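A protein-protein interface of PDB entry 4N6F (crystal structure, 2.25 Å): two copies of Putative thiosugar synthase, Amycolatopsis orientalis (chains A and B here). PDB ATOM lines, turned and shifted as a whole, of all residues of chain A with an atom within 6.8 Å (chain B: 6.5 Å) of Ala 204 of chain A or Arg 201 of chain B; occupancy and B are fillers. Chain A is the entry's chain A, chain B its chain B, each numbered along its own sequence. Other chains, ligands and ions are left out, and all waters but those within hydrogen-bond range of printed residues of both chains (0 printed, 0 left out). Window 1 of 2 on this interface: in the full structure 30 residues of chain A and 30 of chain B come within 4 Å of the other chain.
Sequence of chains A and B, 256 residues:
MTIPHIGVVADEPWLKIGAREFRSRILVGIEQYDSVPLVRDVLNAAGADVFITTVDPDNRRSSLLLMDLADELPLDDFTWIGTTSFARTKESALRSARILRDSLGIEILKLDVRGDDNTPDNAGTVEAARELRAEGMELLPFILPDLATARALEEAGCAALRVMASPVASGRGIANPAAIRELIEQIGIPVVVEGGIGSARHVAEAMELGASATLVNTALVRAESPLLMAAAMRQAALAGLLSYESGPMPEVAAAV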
ATOM      1  N   ILE A 174      -8.885  26.541  13.316  1.00  0.00           N
ATOM      2  CA  ILE A 174      -7.453  26.450  13.586  1.00  0.00           C
ATOM      3  C   ILE A 174      -6.664  27.089  12.444  1.00  0.00           C
ATOM      4  O   ILE A 174      -6.579  26.537  11.356  1.00  0.00           O
ATOM      5  CB  ILE A 174      -7.032  24.991  13.829  1.00  0.00           C
ATOM      6  CG1 ILE A 174      -7.925  24.380  14.925  1.00  0.00           C
ATOM      7  CG2 ILE A 174      -5.562  24.918  14.218  1.00  0.00           C
ATOM      8  CD1 ILE A 174      -7.510  22.993  15.386  1.00  0.00           C
ATOM      9  N   ARG A 181       0.618  21.528  16.136  1.00  0.00           N
ATOM     10  CA  ARG A 181       1.090  20.135  16.150  1.00  0.00           C
ATOM     11  C   ARG A 181       2.551  20.041  16.597  1.00  0.00           C
ATOM     12  O   ARG A 181       2.885  19.247  17.471  1.00  0.00           O
ATOM     13  CB  ARG A 181       0.940  19.489  14.773  1.00  0.00           C
ATOM     14  CG  ARG A 181       1.236  17.990  14.738  1.00  0.00           C
ATOM     15  CD  ARG A 181       1.298  17.462  13.303  1.00  0.00           C
ATOM     16  NE  ARG A 181       0.068  17.739  12.543  1.00  0.00           N
ATOM     17  CZ  ARG A 181      -0.029  18.518  11.456  1.00  0.00           C
ATOM     18  NH1 ARG A 181      -1.214  18.685  10.878  1.00  0.00           N
ATOM     19  NH2 ARG A 181       1.037  19.121  10.927  1.00  0.00           N
ATOM     20  N   SER A 199     -17.178  25.268  15.425  1.00  0.00           N
ATOM     21  CA  SER A 199     -18.066  24.107  15.331  1.00  0.00           C
ATOM     22  C   SER A 199     -17.356  22.804  15.682  1.00  0.00           C
ATOM     23  O   SER A 199     -16.144  22.784  15.922  1.00  0.00           O
ATOM     24  CB  SER A 199     -18.642  24.005  13.919  1.00  0.00           C
ATOM     25  OG  SER A 199     -17.646  23.611  12.987  1.00  0.00           O
ATOM     26  N   ALA A 200     -18.122  21.716  15.675  1.00  0.00           N
ATOM     27  CA  ALA A 200     -17.631  20.398  16.056  1.00  0.00           C
ATOM     28  C   ALA A 200     -16.429  19.905  15.242  1.00  0.00           C
ATOM     29  O   ALA A 200     -15.574  19.201  15.779  1.00  0.00           O
ATOM     30  CB  ALA A 200     -18.757  19.383  15.965  1.00  0.00           C
ATOM     31  N   ARG A 201     -16.368  20.248  13.960  1.00  0.00           N
ATOM     32  CA  ARG A 201     -15.254  19.815  13.124  1.00  0.00           C
ATOM     33  C   ARG A 201     -13.917  20.404  13.573  1.00  0.00           C
ATOM     34  O   ARG A 201     -12.891  19.780  13.376  1.00  0.00           O
ATOM     35  CB  ARG A 201     -15.496  20.132  11.649  1.00  0.00           C
ATOM     36  CG  ARG A 201     -15.237  21.567  11.248  1.00  0.00           C
ATOM     37  CD  ARG A 201     -15.292  21.707   9.737  1.00  0.00           C
ATOM     38  NE  ARG A 201     -15.054  23.080   9.310  1.00  0.00           N
ATOM     39  CZ  ARG A 201     -16.002  23.992   9.088  1.00  0.00           C
ATOM     40  NH1 ARG A 201     -15.655  25.214   8.695  1.00  0.00           N
ATOM     41  NH2 ARG A 201     -17.292  23.698   9.248  1.00  0.00           N
ATOM     42  N   HIS A 202     -13.941  21.603  14.157  1.00  0.00           N
ATOM     43  CA  HIS A 202     -12.732  22.232  14.688  1.00  0.00           C
ATOM     44  C   HIS A 202     -12.227  21.484  15.929  1.00  0.00           C
ATOM     45  O   HIS A 202     -11.018  21.343  16.132  1.00  0.00           O
ATOM     46  CB  HIS A 202     -12.987  23.696  15.054  1.00  0.00           C
ATOM     47  CG  HIS A 202     -13.353  24.575  13.894  1.00  0.00           C
ATOM     48  ND1 HIS A 202     -12.925  24.343  12.603  1.00  0.00           N
ATOM     49  CD2 HIS A 202     -14.075  25.716  13.846  1.00  0.00           C
ATOM     50  CE1 HIS A 202     -13.388  25.294  11.810  1.00  0.00           C
ATOM     51  NE2 HIS A 202     -14.090  26.141  12.540  1.00  0.00           N
ATOM     52  N   VAL A 203     -13.162  21.015  16.752  1.00  0.00           N
ATOM     53  CA  VAL A 203     -12.828  20.228  17.927  1.00  0.00           C
ATOM     54  C   VAL A 203     -12.175  18.921  17.493  1.00  0.00           C
ATOM     55  O   VAL A 203     -11.111  18.581  17.986  1.00  0.00           O
ATOM     56  CB  VAL A 203     -14.063  19.959  18.808  1.00  0.00           C
ATOM     57  CG1 VAL A 203     -13.770  18.925  19.887  1.00  0.00           C
ATOM     58  CG2 VAL A 203     -14.539  21.248  19.439  1.00  0.00           C
ATOM     59  N   ALA A 204     -12.805  18.197  16.565  1.00  0.00           N
ATOM     60  CA  ALA A 204     -12.211  16.962  16.034  1.00  0.00           C
ATOM     61  C   ALA A 204     -10.806  17.219  15.499  1.00  0.00           C
ATOM     62  O   ALA A 204      -9.892  16.434  15.751  1.00  0.00           O
ATOM     63  CB  ALA A 204     -13.080  16.357  14.942  1.00  0.00           C
ATOM     64  N   GLU A 205     -10.641  18.321  14.767  1.00  0.00           N
ATOM     65  CA  GLU A 205      -9.340  18.701  14.237  1.00  0.00           C
ATOM     66  C   GLU A 205      -8.302  18.917  15.354  1.00  0.00           C
ATOM     67  O   GLU A 205      -7.189  18.415  15.265  1.00  0.00           O
ATOM     68  CB  GLU A 205      -9.444  19.956  13.363  1.00  0.00           C
ATOM     69  CG  GLU A 205      -8.135  20.309  12.664  1.00  0.00           C
ATOM     70  CD  GLU A 205      -8.235  21.533  11.777  1.00  0.00           C
ATOM     71  OE1 GLU A 205      -7.199  21.905  11.180  1.00  0.00           O
ATOM     72  OE2 GLU A 205      -9.331  22.132  11.675  1.00  0.00           O
ATOM     73  N   ALA A 206      -8.670  19.654  16.397  1.00  0.00           N
ATOM     74  CA  ALA A 206      -7.750  19.904  17.503  1.00  0.00           C
ATOM     75  C   ALA A 206      -7.222  18.604  18.088  1.00  0.00           C
ATOM     76  O   ALA A 206      -6.031  18.478  18.321  1.00  0.00           O
ATOM     77  CB  ALA A 206      -8.420  20.712  18.594  1.00  0.00           C
ATOM     78  N   MET A 207      -8.105  17.639  18.304  1.00  0.00           N
ATOM     79  CA  MET A 207      -7.710  16.369  18.896  1.00  0.00           C
ATOM     80  C   MET A 207      -6.790  15.574  17.975  1.00  0.00           C
ATOM     81  O   MET A 207      -5.875  14.881  18.450  1.00  0.00           O
ATOM     82  CB  MET A 207      -8.937  15.531  19.248  1.00  0.00           C
ATOM     83  CG  MET A 207      -9.923  16.230  20.170  1.00  0.00           C
ATOM     84  SD  MET A 207      -9.207  16.812  21.713  1.00  0.00           S
ATOM     85  CE  MET A 207      -8.997  15.268  22.574  1.00  0.00           C
ATOM     86  N   GLU A 208      -7.006  15.694  16.664  1.00  0.00           N
ATOM     87  CA  GLU A 208      -6.153  15.009  15.689  1.00  0.00           C
ATOM     88  C   GLU A 208      -4.763  15.628  15.582  1.00  0.00           C
ATOM     89  O   GLU A 208      -3.866  15.013  15.034  1.00  0.00           O
ATOM     90  CB  GLU A 208      -6.830  14.926  14.319  1.00  0.00           C
ATOM     91  CG  GLU A 208      -8.040  14.010  14.357  1.00  0.00           C
ATOM     92  CD  GLU A 208      -8.642  13.707  12.998  1.00  0.00           C
ATOM     93  OE1 GLU A 208      -8.161  14.226  11.965  1.00  0.00           O
ATOM     94  OE2 GLU A 208      -9.611  12.932  12.968  1.00  0.00           O
ATOM     95  N   LEU A 209      -4.585  16.832  16.119  1.00  0.00           N
ATOM     96  CA  LEU A 209      -3.253  17.431  16.255  1.00  0.00           C
ATOM     97  C   LEU A 209      -2.530  16.951  17.530  1.00  0.00           C
ATOM     98  O   LEU A 209      -1.372  17.277  17.729  1.00  0.00           O
ATOM     99  CB  LEU A 209      -3.352  18.959  16.297  1.00  0.00           C
ATOM    100  CG  LEU A 209      -3.972  19.661  15.089  1.00  0.00           C
ATOM    101  CD1 LEU A 209      -3.978  21.154  15.344  1.00  0.00           C
ATOM    102  CD2 LEU A 209      -3.227  19.337  13.805  1.00  0.00           C
ATOM    103  N   THR A 214     -10.217  20.852  24.266  1.00  0.00           N
ATOM    104  CA  THR A 214     -10.578  22.084  23.599  1.00  0.00           C
ATOM    105  C   THR A 214     -11.431  22.923  24.538  1.00  0.00           C
ATOM    106  O   THR A 214     -12.286  22.390  25.243  1.00  0.00           O
ATOM    107  CB  THR A 214     -11.393  21.778  22.333  1.00  0.00           C
ATOM    108  OG1 THR A 214     -10.641  20.889  21.504  1.00  0.00           O
ATOM    109  CG2 THR A 214     -11.681  23.040  21.550  1.00  0.00           C
ATOM    110  N   MET A 233     -20.090  18.802  20.154  1.00  0.00           N
ATOM    111  CA  MET A 233     -18.687  18.990  20.477  1.00  0.00           C
ATOM    112  C   MET A 233     -18.133  17.897  21.404  1.00  0.00           C
ATOM    113  O   MET A 233     -16.989  17.468  21.228  1.00  0.00           O
ATOM    114  CB  MET A 233     -18.474  20.381  21.061  1.00  0.00           C
ATOM    115  CG  MET A 233     -18.453  21.427  19.965  1.00  0.00           C
ATOM    116  SD  MET A 233     -18.221  23.073  20.618  1.00  0.00           S
ATOM    117  CE  MET A 233     -17.950  23.950  19.081  1.00  0.00           C
ATOM    118  N   ALA A 236     -17.571  15.060  19.098  1.00  0.00           N
ATOM    119  CA  ALA A 236     -16.463  15.354  18.200  1.00  0.00           C
ATOM    120  C   ALA A 236     -15.104  15.212  18.886  1.00  0.00           C
ATOM    121  O   ALA A 236     -14.121  14.799  18.261  1.00  0.00           O
ATOM    122  CB  ALA A 236     -16.610  16.751  17.622  1.00  0.00           C
ATOM    123  N   ALA A 237     -15.053  15.589  20.157  1.00  0.00           N
ATOM    124  CA  ALA A 237     -13.836  15.475  20.958  1.00  0.00           C
ATOM    125  C   ALA A 237     -13.464  14.007  21.134  1.00  0.00           C
ATOM    126  O   ALA A 237     -12.307  13.626  20.999  1.00  0.00           O
ATOM    127  CB  ALA A 237     -14.036  16.139  22.316  1.00  0.00           C
ATOM    128  N   ALA A 239     -14.562  11.427  19.175  1.00  0.00           N
ATOM    129  CA  ALA A 239     -14.213  10.900  17.850  1.00  0.00           C
ATOM    130  C   ALA A 239     -12.805  11.297  17.453  1.00  0.00           C
ATOM    131  O   ALA A 239     -12.075  10.509  16.870  1.00  0.00           O
ATOM    132  CB  ALA A 239     -15.188  11.398  16.788  1.00  0.00           C
ATOM    133  N   GLY A 240     -12.443  12.541  17.732  1.00  0.00           N
ATOM    134  CA  GLY A 240     -11.129  13.060  17.382  1.00  0.00           C
ATOM    135  C   GLY A 240     -10.019  12.370  18.146  1.00  0.00           C
ATOM    136  O   GLY A 240      -8.953  12.117  17.603  1.00  0.00           O
ATOM    137  N   LEU A 241     -10.276  12.098  19.420  1.00  0.00           N
ATOM    138  CA  LEU A 241      -9.336  11.389  20.271  1.00  0.00           C
ATOM    139  C   LEU A 241      -9.121   9.981  19.724  1.00  0.00           C
ATOM    140  O   LEU A 241      -7.985   9.578  19.470  1.00  0.00           O
ATOM    141  CB  LEU A 241      -9.857  11.346  21.707  1.00  0.00           C
ATOM    142  CG  LEU A 241      -8.997  10.606  22.734  1.00  0.00           C
ATOM    143  CD1 LEU A 241      -7.719  11.382  23.014  1.00  0.00           C
ATOM    144  CD2 LEU A 241      -9.777  10.368  24.021  1.00  0.00           C
ATOM    145  N   SER A 243      -9.679   8.814  16.820  1.00  0.00           N
ATOM    146  CA  SER A 243      -9.058   8.914  15.513  1.00  0.00           C
ATOM    147  C   SER A 243      -7.559   9.178  15.659  1.00  0.00           C
ATOM    148  O   SER A 243      -6.744   8.545  14.988  1.00  0.00           O
ATOM    149  CB  SER A 243      -9.747  10.022  14.695  1.00  0.00           C
ATOM    150  OG  SER A 243      -9.041  10.350  13.518  1.00  0.00           O
ATOM    151  N   GLU A 251      -1.116  12.296   5.245  1.00  0.00           N
ATOM    152  CA  GLU A 251      -1.668  13.017   4.106  1.00  0.00           C
ATOM    153  C   GLU A 251      -0.665  13.060   2.955  1.00  0.00           C
ATOM    154  O   GLU A 251       0.473  13.487   3.135  1.00  0.00           O
ATOM    155  CB  GLU A 251      -2.065  14.434   4.535  1.00  0.00           C
ATOM    156  CG  GLU A 251      -2.332  15.406   3.396  1.00  0.00           C
ATOM    157  CD  GLU A 251      -2.975  16.704   3.861  1.00  0.00           C
ATOM    158  OE1 GLU A 251      -3.167  17.601   3.016  1.00  0.00           O
ATOM    159  OE2 GLU A 251      -3.291  16.831   5.064  1.00  0.00           O
ATOM    160  N   GLY B 171      -5.905  10.912   1.427  1.00  0.00           N
ATOM    161  CA  GLY B 171      -6.149  11.318   2.814  1.00  0.00           C
ATOM    162  C   GLY B 171      -6.146  12.826   3.040  1.00  0.00           C
ATOM    163  O   GLY B 171      -5.992  13.274   4.178  1.00  0.00           O
ATOM    164  N   ARG B 172      -6.341  13.602   1.970  1.00  0.00           N
ATOM    165  CA  ARG B 172      -6.317  15.075   2.034  1.00  0.00           C
ATOM    166  C   ARG B 172      -7.618  15.712   2.560  1.00  0.00           C
ATOM    167  O   ARG B 172      -7.662  16.911   2.826  1.00  0.00           O
ATOM    168  CB  ARG B 172      -5.983  15.669   0.656  1.00  0.00           C
ATOM    169  CG  ARG B 172      -4.525  15.520   0.254  1.00  0.00           C
ATOM    170  CD  ARG B 172      -4.301  15.808  -1.229  1.00  0.00           C
ATOM    171  NE  ARG B 172      -2.875  15.968  -1.536  1.00  0.00           N
ATOM    172  CZ  ARG B 172      -2.291  15.704  -2.713  1.00  0.00           C
ATOM    173  NH1 ARG B 172      -2.993  15.246  -3.751  1.00  0.00           N
ATOM    174  NH2 ARG B 172      -0.977  15.895  -2.850  1.00  0.00           N
ATOM    175  N   GLY B 173      -8.673  14.922   2.705  1.00  0.00           N
ATOM    176  CA  GLY B 173      -9.945  15.445   3.193  1.00  0.00           C
ATOM    177  C   GLY B 173     -10.697  16.174   2.098  1.00  0.00           C
ATOM    178  O   GLY B 173     -10.761  15.699   0.958  1.00  0.00           O
ATOM    179  N   SER B 199      -9.383  10.857   7.933  1.00  0.00           N
ATOM    180  CA  SER B 199      -9.601  10.744   9.374  1.00  0.00           C
ATOM    181  C   SER B 199     -10.984  11.217   9.769  1.00  0.00           C
ATOM    182  O   SER B 199     -11.770  11.647   8.923  1.00  0.00           O
ATOM    183  CB  SER B 199      -8.537  11.548  10.121  1.00  0.00           C
ATOM    184  OG  SER B 199      -8.614  12.921   9.785  1.00  0.00           O
ATOM    185  N   ALA B 200     -11.269  11.141  11.067  1.00  0.00           N
ATOM    186  CA  ALA B 200     -12.582  11.474  11.603  1.00  0.00           C
ATOM    187  C   ALA B 200     -12.985  12.931  11.392  1.00  0.00           C
ATOM    188  O   ALA B 200     -14.166  13.214  11.187  1.00  0.00           O
ATOM    189  CB  ALA B 200     -12.645  11.134  13.082  1.00  0.00           C
ATOM    190  N   ARG B 201     -12.025  13.851  11.446  1.00  0.00           N
ATOM    191  CA  ARG B 201     -12.347  15.273  11.299  1.00  0.00           C
ATOM    192  C   ARG B 201     -12.893  15.578   9.911  1.00  0.00           C
ATOM    193  O   ARG B 201     -13.719  16.471   9.757  1.00  0.00           O
ATOM    194  CB  ARG B 201     -11.140  16.164  11.597  1.00  0.00           C
ATOM    195  CG  ARG B 201     -10.181  16.376  10.439  1.00  0.00           C
ATOM    196  CD  ARG B 201      -8.987  17.191  10.885  1.00  0.00           C
ATOM    197  NE  ARG B 201      -7.809  16.912  10.072  1.00  0.00           N
ATOM    198  CZ  ARG B 201      -7.472  17.570   8.969  1.00  0.00           C
ATOM    199  NH1 ARG B 201      -6.378  17.208   8.313  1.00  0.00           N
ATOM    200  NH2 ARG B 201      -8.224  18.572   8.506  1.00  0.00           N
ATOM    201  N   HIS B 202     -12.435  14.825   8.914  1.00  0.00           N
ATOM    202  CA  HIS B 202     -12.915  14.980   7.543  1.00  0.00           C
ATOM    203  C   HIS B 202     -14.378  14.564   7.408  1.00  0.00           C
ATOM    204  O   HIS B 202     -15.130  15.179   6.648  1.00  0.00           O
ATOM    205  CB  HIS B 202     -12.044  14.189   6.580  1.00  0.00           C
ATOM    206  CG  HIS B 202     -10.630  14.677   6.514  1.00  0.00           C
ATOM    207  ND1 HIS B 202      -9.572  13.851   6.225  1.00  0.00           N
ATOM    208  CD2 HIS B 202     -10.099  15.903   6.723  1.00  0.00           C
ATOM    209  CE1 HIS B 202      -8.449  14.541   6.246  1.00  0.00           C
ATOM    210  NE2 HIS B 202      -8.740  15.791   6.543  1.00  0.00           N
ATOM    211  N   VAL B 203     -14.776  13.542   8.165  1.00  0.00           N
ATOM    212  CA  VAL B 203     -16.160  13.086   8.198  1.00  0.00           C
ATOM    213  C   VAL B 203     -17.059  14.141   8.849  1.00  0.00           C
ATOM    214  O   VAL B 203     -18.107  14.492   8.304  1.00  0.00           O
ATOM    215  CB  VAL B 203     -16.293  11.742   8.937  1.00  0.00           C
ATOM    216  CG1 VAL B 203     -17.749  11.387   9.178  1.00  0.00           C
ATOM    217  CG2 VAL B 203     -15.613  10.629   8.148  1.00  0.00           C
ATOM    218  N   ALA B 204     -16.644  14.639  10.016  1.00  0.00           N
ATOM    219  CA  ALA B 204     -17.373  15.692  10.713  1.00  0.00           C
ATOM    220  C   ALA B 204     -17.560  16.906   9.803  1.00  0.00           C
ATOM    221  O   ALA B 204     -18.634  17.478   9.749  1.00  0.00           O
ATOM    222  CB  ALA B 204     -16.653  16.085  11.993  1.00  0.00           C
ATOM    223  N   GLU B 205     -16.516  17.263   9.065  1.00  0.00           N
ATOM    224  CA  GLU B 205     -16.570  18.386   8.150  1.00  0.00           C
ATOM    225  C   GLU B 205     -17.608  18.166   7.038  1.00  0.00           C
ATOM    226  O   GLU B 205     -18.447  19.030   6.793  1.00  0.00           O
ATOM    227  CB  GLU B 205     -15.188  18.646   7.557  1.00  0.00           C
ATOM    228  CG  GLU B 205     -15.126  19.871   6.653  1.00  0.00           C
ATOM    229  CD  GLU B 205     -13.742  20.109   6.077  1.00  0.00           C
ATOM    230  OE1 GLU B 205     -13.592  21.070   5.297  1.00  0.00           O
ATOM    231  OE2 GLU B 205     -12.804  19.336   6.391  1.00  0.00           O
ATOM    232  N   ALA B 206     -17.561  17.004   6.394  1.00  0.00           N
ATOM    233  CA  ALA B 206     -18.538  16.643   5.354  1.00  0.00           C
ATOM    234  C   ALA B 206     -19.978  16.788   5.837  1.00  0.00           C
ATOM    235  O   ALA B 206     -20.837  17.308   5.128  1.00  0.00           O
ATOM    236  CB  ALA B 206     -18.292  15.222   4.879  1.00  0.00           C
ATOM    237  N   MET B 233     -14.901   7.282  13.081  1.00  0.00           N
ATOM    238  CA  MET B 233     -15.639   7.874  11.976  1.00  0.00           C
ATOM    239  C   MET B 233     -17.153   7.811  12.185  1.00  0.00           C
ATOM    240  O   MET B 233     -17.858   8.771  11.891  1.00  0.00           O
ATOM    241  CB  MET B 233     -15.212   7.230  10.682  1.00  0.00           C
ATOM    242  CG  MET B 233     -13.873   7.775  10.241  1.00  0.00           C
ATOM    243  SD  MET B 233     -13.312   6.918   8.790  1.00  0.00           S
ATOM    244  CE  MET B 233     -12.011   8.021   8.265  1.00  0.00           C
ATOM    245  N   ALA B 236     -17.844  10.648  14.639  1.00  0.00           N
ATOM    246  CA  ALA B 236     -17.699  11.955  13.980  1.00  0.00           C
ATOM    247  C   ALA B 236     -18.891  12.307  13.076  1.00  0.00           C
ATOM    248  O   ALA B 236     -19.251  13.472  12.957  1.00  0.00           O
ATOM    249  CB  ALA B 236     -16.415  11.996  13.169  1.00  0.00           C
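OE1 of Glu 208 of chain A sits at hydrogen-bond distance from OG of Ser 199 of chain B. The side-chain carboxylate (OE2) of Glu 208 of chain A is in hydrogen-bond range of the backbone NH (N) of Ala 200 of chain B, at 3.1 Å. The guanidinium group of Arg 201 of chain B is in salt-bridge range of the side-chain carboxylate of Glu 208 of chain A, 3.3 Å away. The side-chain hydroxyl (OG) of Ser 243 of chain A sits at hydrogen-bond distance from the backbone NH (N) of Ala 200 of chain B (3.4 Å).
The side-chain carboxylate (OE2) of Glu 208 of chain A is in hydrogen-bond range of the side-chain hydroxyl (OG) of Ser 243 of chain A (2.7 Å). A ring nitrogen (ND1) of His 202 of chain B lies within hydrogen-bond range of the backbone NH (N) of Ser 199 of chain B (3.5 Å). NH1 of Arg 201 of chain B sits close to NE2 of His 202 of chain B, at 3.3 Å.
Among the printed residues, pairs that only touch across the chains: Ala 239 of chain A with Ala 236 of chain B (3.5 Å), Arg 201 of chain A with Glu 205 of chain B (3.6 Å), Ser 243 of chain A with Ser 199 of chain B (3.6 Å), Glu 205 of chain A with Arg 201 of chain B (3.7 Å), Glu 251 of chain A with Arg 172 of chain B (3.7 Å), Ala 204 of chain A with Arg 201 of chain B (3.9 Å) and Ala 239 of chain A with Ala 200 of chain B (3.9 Å).
Ala 204 of chain A touches just one residue of chain B: Arg 201. Arg 201 of chain B touches just these residues of chain A: Ala 204, Glu 205 and Glu 208. Of the printed residues of chain A, Arg 172 of chain B touches Glu 251 (3.7 Å). Of the printed residues of chain A, Ala 200 of chain B touches Glu 208 (3.1 Å), Ala 239 (3.9 Å) and Ser 243 (3.4 Å). Printed residues of chain B within 4 Å of Glu 205 of chain A: Arg 201. Printed residues of chain B within 4 Å of Glu 251 of chain A: Arg 172. His 202 of chain B touches none of the printed residues of chain A. Ser 199 of chain A touches none of the printed residues of chain B.
Of the 22 printed residues of chain A, 7 touch a printed residue of chain B. Printed residues of chain A that touch a printed residue of chain B: Arg 201, Ala 204, Glu 205, Glu 208, Ala 239, Ser 243 and Glu 251. Among the printed residues, Asp or Glu carboxylates within 4 Å of a Lys or Arg side-chain nitrogen of the other chain: Glu 208 of chain A with Arg 201 of chain B (3.3 Å).
Arg 201 of chain A touches Glu 205 of chain B, and with the chains exchanged Glu 205 of chain A touches Arg 201 of chain B. Ala 204 of chain A touches Arg 201 of chain B, but with the chains exchanged Arg 201 of chain A does not touch Ala 204 of chain B (4.1 Å). Of the 11 pairs that touch across the chains among the printed residues, 2 have their exchanged pair printed and touching as well.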
